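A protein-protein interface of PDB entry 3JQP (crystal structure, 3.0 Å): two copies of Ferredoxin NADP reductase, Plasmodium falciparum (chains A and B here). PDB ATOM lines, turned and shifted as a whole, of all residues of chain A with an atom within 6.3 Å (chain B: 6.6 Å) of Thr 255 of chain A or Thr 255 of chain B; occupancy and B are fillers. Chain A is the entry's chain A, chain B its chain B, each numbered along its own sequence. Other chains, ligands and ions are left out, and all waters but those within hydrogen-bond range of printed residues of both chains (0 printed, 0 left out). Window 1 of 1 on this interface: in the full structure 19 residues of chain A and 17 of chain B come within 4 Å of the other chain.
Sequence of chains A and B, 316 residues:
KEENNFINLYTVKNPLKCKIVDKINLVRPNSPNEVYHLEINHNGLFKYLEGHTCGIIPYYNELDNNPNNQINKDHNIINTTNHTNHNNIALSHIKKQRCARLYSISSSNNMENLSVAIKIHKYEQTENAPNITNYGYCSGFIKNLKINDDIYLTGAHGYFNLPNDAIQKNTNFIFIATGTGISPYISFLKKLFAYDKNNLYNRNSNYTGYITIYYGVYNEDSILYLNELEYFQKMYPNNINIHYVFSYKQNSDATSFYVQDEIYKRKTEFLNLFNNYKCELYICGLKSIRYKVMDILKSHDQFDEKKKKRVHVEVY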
ATOM      1  N   GLN A 250       6.339   4.655   3.689  1.00  0.00           N
ATOM      2  CA  GLN A 250       7.201   5.602   4.399  1.00  0.00           C
ATOM      3  C   GLN A 250       7.555   6.857   3.596  1.00  0.00           C
ATOM      4  O   GLN A 250       8.285   7.724   4.080  1.00  0.00           O
ATOM      5  CB  GLN A 250       8.477   4.909   4.879  1.00  0.00           C
ATOM      6  CG  GLN A 250       8.231   3.794   5.882  1.00  0.00           C
ATOM      7  CD  GLN A 250       7.478   4.269   7.112  1.00  0.00           C
ATOM      8  OE1 GLN A 250       7.160   5.452   7.240  1.00  0.00           O
ATOM      9  NE2 GLN A 250       7.186   3.345   8.023  1.00  0.00           N
ATOM     10  N   ASN A 251       7.040   6.950   2.373  1.00  0.00           N
ATOM     11  CA  ASN A 251       7.305   8.103   1.517  1.00  0.00           C
ATOM     12  C   ASN A 251       6.952   9.405   2.201  1.00  0.00           C
ATOM     13  O   ASN A 251       7.688  10.397   2.115  1.00  0.00           O
ATOM     14  CB  ASN A 251       6.460   8.008   0.254  1.00  0.00           C
ATOM     15  CG  ASN A 251       7.059   7.092  -0.775  1.00  0.00           C
ATOM     16  OD1 ASN A 251       8.044   6.396  -0.451  1.00  0.00           O
ATOM     17  ND2 ASN A 251       6.542   7.070  -1.913  1.00  0.00           N
ATOM     18  N   SER A 252       5.797   9.397   2.860  1.00  0.00           N
ATOM     19  CA  SER A 252       5.258  10.599   3.464  1.00  0.00           C
ATOM     20  C   SER A 252       6.003  10.968   4.739  1.00  0.00           C
ATOM     21  O   SER A 252       7.130  10.521   4.968  1.00  0.00           O
ATOM     22  CB  SER A 252       3.755  10.437   3.734  1.00  0.00           C
ATOM     23  OG  SER A 252       3.465   9.182   4.332  1.00  0.00           O
ATOM     24  N   ASP A 253       5.367  11.790   5.564  1.00  0.00           N
ATOM     25  CA  ASP A 253       6.029  12.319   6.750  1.00  0.00           C
ATOM     26  C   ASP A 253       6.253  11.233   7.799  1.00  0.00           C
ATOM     27  O   ASP A 253       5.586  11.208   8.833  1.00  0.00           O
ATOM     28  CB  ASP A 253       5.211  13.467   7.339  1.00  0.00           C
ATOM     29  CG  ASP A 253       3.828  13.027   7.779  1.00  0.00           C
ATOM     30  OD1 ASP A 253       3.553  11.806   7.774  1.00  0.00           O
ATOM     31  OD2 ASP A 253       3.013  13.905   8.135  1.00  0.00           O
ATOM     32  N   THR A 255       9.848   8.450   8.582  1.00  0.00           N
ATOM     33  CA  THR A 255      11.189   7.907   8.371  1.00  0.00           C
ATOM     34  C   THR A 255      11.144   6.579   7.627  1.00  0.00           C
ATOM     35  O   THR A 255      10.076   5.994   7.453  1.00  0.00           O
ATOM     36  CB  THR A 255      11.916   7.685   9.697  1.00  0.00           C
ATOM     37  OG1 THR A 255      11.154   6.785  10.512  1.00  0.00           O
ATOM     38  CG2 THR A 255      12.091   9.004  10.428  1.00  0.00           C
ATOM     39  N   SER A 256      12.307   6.103   7.197  1.00  0.00           N
ATOM     40  CA  SER A 256      12.381   4.856   6.443  1.00  0.00           C
ATOM     41  C   SER A 256      12.050   3.641   7.300  1.00  0.00           C
ATOM     42  O   SER A 256      12.448   3.554   8.461  1.00  0.00           O
ATOM     43  CB  SER A 256      13.762   4.687   5.807  1.00  0.00           C
ATOM     44  OG  SER A 256      13.938   5.580   4.721  1.00  0.00           O
ATOM     45  N   PHE A 257      11.314   2.704   6.712  1.00  0.00           N
ATOM     46  CA  PHE A 257      10.980   1.447   7.369  1.00  0.00           C
ATOM     47  C   PHE A 257      11.112   0.313   6.359  1.00  0.00           C
ATOM     48  O   PHE A 257      10.358   0.244   5.390  1.00  0.00           O
ATOM     49  CB  PHE A 257       9.557   1.498   7.930  1.00  0.00           C
ATOM     50  CG  PHE A 257       9.207   0.331   8.811  1.00  0.00           C
ATOM     51  CD1 PHE A 257       9.486   0.363  10.169  1.00  0.00           C
ATOM     52  CD2 PHE A 257       8.598  -0.795   8.286  1.00  0.00           C
ATOM     53  CE1 PHE A 257       9.166  -0.708  10.985  1.00  0.00           C
ATOM     54  CE2 PHE A 257       8.276  -1.870   9.096  1.00  0.00           C
ATOM     55  CZ  PHE A 257       8.561  -1.827  10.448  1.00  0.00           C
ATOM     56  N   ASP A 261      13.458  -3.671   9.663  1.00  0.00           N
ATOM     57  CA  ASP A 261      12.815  -2.946  10.746  1.00  0.00           C
ATOM     58  C   ASP A 261      11.683  -3.793  11.333  1.00  0.00           C
ATOM     59  O   ASP A 261      11.582  -3.949  12.552  1.00  0.00           O
ATOM     60  CB  ASP A 261      12.308  -1.585  10.271  1.00  0.00           C
ATOM     61  CG  ASP A 261      13.435  -0.654   9.865  1.00  0.00           C
ATOM     62  OD1 ASP A 261      14.553  -0.797  10.402  1.00  0.00           O
ATOM     63  OD2 ASP A 261      13.195   0.225   9.010  1.00  0.00           O
ATOM     64  N   TYR A 264      13.008  -6.298  13.515  1.00  0.00           N
ATOM     65  CA  TYR A 264      13.374  -5.723  14.804  1.00  0.00           C
ATOM     66  C   TYR A 264      12.119  -5.452  15.624  1.00  0.00           C
ATOM     67  O   TYR A 264      12.012  -5.886  16.771  1.00  0.00           O
ATOM     68  CB  TYR A 264      14.197  -4.442  14.630  1.00  0.00           C
ATOM     69  CG  TYR A 264      14.481  -3.702  15.925  1.00  0.00           C
ATOM     70  CD1 TYR A 264      15.471  -4.137  16.803  1.00  0.00           C
ATOM     71  CD2 TYR A 264      13.762  -2.562  16.265  1.00  0.00           C
ATOM     72  CE1 TYR A 264      15.732  -3.459  17.987  1.00  0.00           C
ATOM     73  CE2 TYR A 264      14.016  -1.877  17.444  1.00  0.00           C
ATOM     74  CZ  TYR A 264      15.001  -2.328  18.301  1.00  0.00           C
ATOM     75  OH  TYR A 264      15.250  -1.644  19.470  1.00  0.00           O
ATOM     76  N   LYS A 292      21.427  -5.326  11.008  1.00  0.00           N
ATOM     77  CA  LYS A 292      20.436  -5.164  12.067  1.00  0.00           C
ATOM     78  C   LYS A 292      19.695  -6.444  12.423  1.00  0.00           C
ATOM     79  O   LYS A 292      18.906  -6.461  13.374  1.00  0.00           O
ATOM     80  CB  LYS A 292      19.414  -4.092  11.715  1.00  0.00           C
ATOM     81  CG  LYS A 292      18.239  -4.089  12.672  1.00  0.00           C
ATOM     82  CD  LYS A 292      17.203  -3.072  12.261  1.00  0.00           C
ATOM     83  CE  LYS A 292      17.810  -1.683  12.192  1.00  0.00           C
ATOM     84  NZ  LYS A 292      16.835  -0.677  11.685  1.00  0.00           N
ATOM     85  N   LYS B 249      23.607   3.514  15.108  1.00  0.00           N
ATOM     86  CA  LYS B 249      22.937   4.325  16.126  1.00  0.00           C
ATOM     87  C   LYS B 249      22.880   3.633  17.491  1.00  0.00           C
ATOM     88  O   LYS B 249      22.621   4.272  18.513  1.00  0.00           O
ATOM     89  CB  LYS B 249      21.527   4.697  15.657  1.00  0.00           C
ATOM     90  CG  LYS B 249      20.776   3.536  15.023  1.00  0.00           C
ATOM     91  CD  LYS B 249      19.718   4.029  14.044  1.00  0.00           C
ATOM     92  CE  LYS B 249      19.471   2.990  12.962  1.00  0.00           C
ATOM     93  NZ  LYS B 249      19.418   1.610  13.520  1.00  0.00           N
ATOM     94  N   THR B 255      13.143   1.290  13.744  1.00  0.00           N
ATOM     95  CA  THR B 255      13.065   1.959  12.448  1.00  0.00           C
ATOM     96  C   THR B 255      14.451   2.396  11.971  1.00  0.00           C
ATOM     97  O   THR B 255      15.390   2.495  12.763  1.00  0.00           O
ATOM     98  CB  THR B 255      12.151   3.199  12.504  1.00  0.00           C
ATOM     99  OG1 THR B 255      12.954   4.383  12.603  1.00  0.00           O
ATOM    100  CG2 THR B 255      11.204   3.116  13.695  1.00  0.00           C
ATOM    101  N   SER B 256      14.569   2.657  10.672  1.00  0.00           N
ATOM    102  CA  SER B 256      15.832   3.095  10.080  1.00  0.00           C
ATOM    103  C   SER B 256      15.750   4.534   9.566  1.00  0.00           C
ATOM    104  O   SER B 256      14.671   5.033   9.245  1.00  0.00           O
ATOM    105  CB  SER B 256      16.262   2.146   8.957  1.00  0.00           C
ATOM    106  OG  SER B 256      15.259   2.033   7.963  1.00  0.00           O
ATOM    107  N   PHE B 257      16.903   5.193   9.492  1.00  0.00           N
ATOM    108  CA  PHE B 257      16.959   6.600   9.112  1.00  0.00           C
ATOM    109  C   PHE B 257      18.130   6.846   8.182  1.00  0.00           C
ATOM    110  O   PHE B 257      19.279   6.609   8.546  1.00  0.00           O
ATOM    111  CB  PHE B 257      17.138   7.456  10.360  1.00  0.00           C
ATOM    112  CG  PHE B 257      16.806   8.897  10.156  1.00  0.00           C
ATOM    113  CD1 PHE B 257      15.514   9.346  10.342  1.00  0.00           C
ATOM    114  CD2 PHE B 257      17.784   9.806   9.797  1.00  0.00           C
ATOM    115  CE1 PHE B 257      15.199  10.673  10.167  1.00  0.00           C
ATOM    116  CE2 PHE B 257      17.475  11.135   9.621  1.00  0.00           C
ATOM    117  CZ  PHE B 257      16.180  11.569   9.806  1.00  0.00           C
ATOM    118  N   TYR B 258      17.848   7.332   6.981  1.00  0.00           N
ATOM    119  CA  TYR B 258      18.911   7.577   6.022  1.00  0.00           C
ATOM    120  C   TYR B 258      18.963   9.028   5.592  1.00  0.00           C
ATOM    121  O   TYR B 258      18.457   9.911   6.281  1.00  0.00           O
ATOM    122  CB  TYR B 258      18.762   6.674   4.799  1.00  0.00           C
ATOM    123  CG  TYR B 258      18.975   5.220   5.112  1.00  0.00           C
ATOM    124  CD1 TYR B 258      20.162   4.783   5.676  1.00  0.00           C
ATOM    125  CD2 TYR B 258      17.992   4.284   4.841  1.00  0.00           C
ATOM    126  CE1 TYR B 258      20.362   3.459   5.965  1.00  0.00           C
ATOM    127  CE2 TYR B 258      18.183   2.957   5.124  1.00  0.00           C
ATOM    128  CZ  TYR B 258      19.369   2.550   5.686  1.00  0.00           C
ATOM    129  OH  TYR B 258      19.563   1.220   5.973  1.00  0.00           O
ATOM    130  N   ASP B 261      15.660  10.825   4.712  1.00  0.00           N
ATOM    131  CA  ASP B 261      14.920  11.100   5.935  1.00  0.00           C
ATOM    132  C   ASP B 261      15.435  12.365   6.611  1.00  0.00           C
ATOM    133  O   ASP B 261      14.661  13.130   7.180  1.00  0.00           O
ATOM    134  CB  ASP B 261      15.013   9.906   6.882  1.00  0.00           C
ATOM    135  CG  ASP B 261      14.648   8.600   6.204  1.00  0.00           C
ATOM    136  OD1 ASP B 261      15.302   7.577   6.495  1.00  0.00           O
ATOM    137  OD2 ASP B 261      13.713   8.598   5.373  1.00  0.00           O
ATOM    138  N   LYS B 292      12.092   9.725  -2.447  1.00  0.00           N
ATOM    139  CA  LYS B 292      11.735  10.498  -1.267  1.00  0.00           C
ATOM    140  C   LYS B 292      12.143  11.970  -1.369  1.00  0.00           C
ATOM    141  O   LYS B 292      11.539  12.827  -0.728  1.00  0.00           O
ATOM    142  CB  LYS B 292      12.298   9.851   0.001  1.00  0.00           C
ATOM    143  CG  LYS B 292      11.655  10.352   1.288  1.00  0.00           C
ATOM    144  CD  LYS B 292      12.013   9.457   2.465  1.00  0.00           C
ATOM    145  CE  LYS B 292      11.698  10.125   3.793  1.00  0.00           C
ATOM    146  NZ  LYS B 292      10.233  10.362   3.969  1.00  0.00           N
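Of chain A, only Thr 255 (3.7 Å), Asp 261 (3.6 Å) and Lys 292 (3.6 Å) come within 4 Å of Thr 255 of chain B.
Printed residues of chain B within 4 Å of Ser 256 of chain A: Ser 256 (2.8 Å) and Asp 261 (3.0 Å).
Of the printed residues of chain A, Asp 261 of chain B touches Thr 255 and Ser 256.
Printed residues of chain B within 4 Å of Ser 252 of chain A: Lys 292 (3.3 Å).
Of the printed residues of chain B, Lys 292 of chain A touches Lys 249 (3.9 Å), Thr 255 (3.6 Å) and Ser 256 (3.97 Å).
Of the printed residues of chain A, Ser 256 of chain B touches Thr 255, Ser 256, Asp 261 and Lys 292.
Tyr 264 of chain A touches none of the printed residues of chain B.
Phe 257 of chain A touches none of the printed residues of chain B.
The nearest residue of chain B that does not touch Thr 255 of chain A is Lys 292 of chain B (5.0 Å).
The nearest printed residue of chain B that does not touch Asp 261 of chain A is Phe 257 of chain B (6.2 Å).
Printed residues of chain A that touch a printed residue of chain B: Gln 250, Asn 251, Ser 252, Thr 255, Ser 256, Asp 261 and Lys 292.
Of the 7 printed residues of chain B, 6 touch a printed residue of chain A.
Printed residues of chain B that touch a printed residue of chain A: Lys 249, Thr 255, Ser 256, Phe 257, Asp 261 and Lys 292.
Hydrophobic or aromatic side chains of chain B within 4 Å of the printed part of chain A: Phe 257.
Along chain B the printed residues that touch a printed residue of chain A span positions 249 to 292.
Among the printed residues, 14 pairs touch across the chains.
Among the printed residues, no Asp or Glu carboxylate lies within 4 Å of a Lys or Arg side-chain nitrogen of the other chain.
The side-chain amino group (NZ) of Lys 292 of chain B is in hydrogen-bond range of the backbone carbonyl oxygen (O) of Gln 250 of chain A, at 3.3 Å.
NZ of Lys 292 of chain B lies within hydrogen-bond range of O of Asn 251 of chain A.
NZ of Lys 292 of chain B lies within hydrogen-bond range of O of Ser 252 of chain A.
The backbone NH of Ser 256 of chain B sits at hydrogen-bond distance from the backbone carbonyl oxygen of Ser 256 of chain A, at 3.2 Å.
OG of Ser 256 of chain A sits at hydrogen-bond distance from OD1 of Asp 261 of chain B, at 3.0 Å.
The side-chain carboxylate (OD2) of Asp 261 of chain A lies within hydrogen-bond range of the side-chain hydroxyl (OG) of Ser 256 of chain B (2.9 Å).
Among the printed residues, merely in contact across the chains: Thr 255 of chain A with Thr 255 of chain B, Thr 255 of chain A with Ser 256 of chain B, Thr 255 of chain A with Phe 257 of chain B, Thr 255 of chain A with Asp 261 of chain B, Asp 261 of chain A with Thr 255 of chain B, Lys 292 of chain A with Lys 249 of chain B, Lys 292 of chain A with Thr 255 of chain B and Lys 292 of chain A with Ser 256 of chain B.
Thr 255 of chain B touches its own counterpart, Thr 255 of chain A.
Ser 256 of chain A touches its own counterpart, Ser 256 of chain B.
Ser 256 of chain A touches Asp 261 of chain B, and with the chains exchanged Asp 261 of chain A touches Ser 256 of chain B.
Lys 292 of chain A touches Ser 256 of chain B, but with the chains exchanged Ser 256 of chain A does not touch Lys 292 of chain B (4.9 Å).
Positions printed for both chains: 255, 256, 257, 261 and 292.
Of the 14 pairs that touch across the chains among the printed residues, 6 have their exchanged pair printed and touching as well.
OE1 of Gln 250 of chain A lies close to O of Thr 255 of chain A.
OD1 of Asp 261 of chain A is in salt-bridge range of NZ of Lys 292 of chain A, at 2.6 Å.
The backbone NH (N) of Tyr 258 of chain B lies within hydrogen-bond range of the side-chain carboxylate (OD1) of Asp 261 of chain B.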
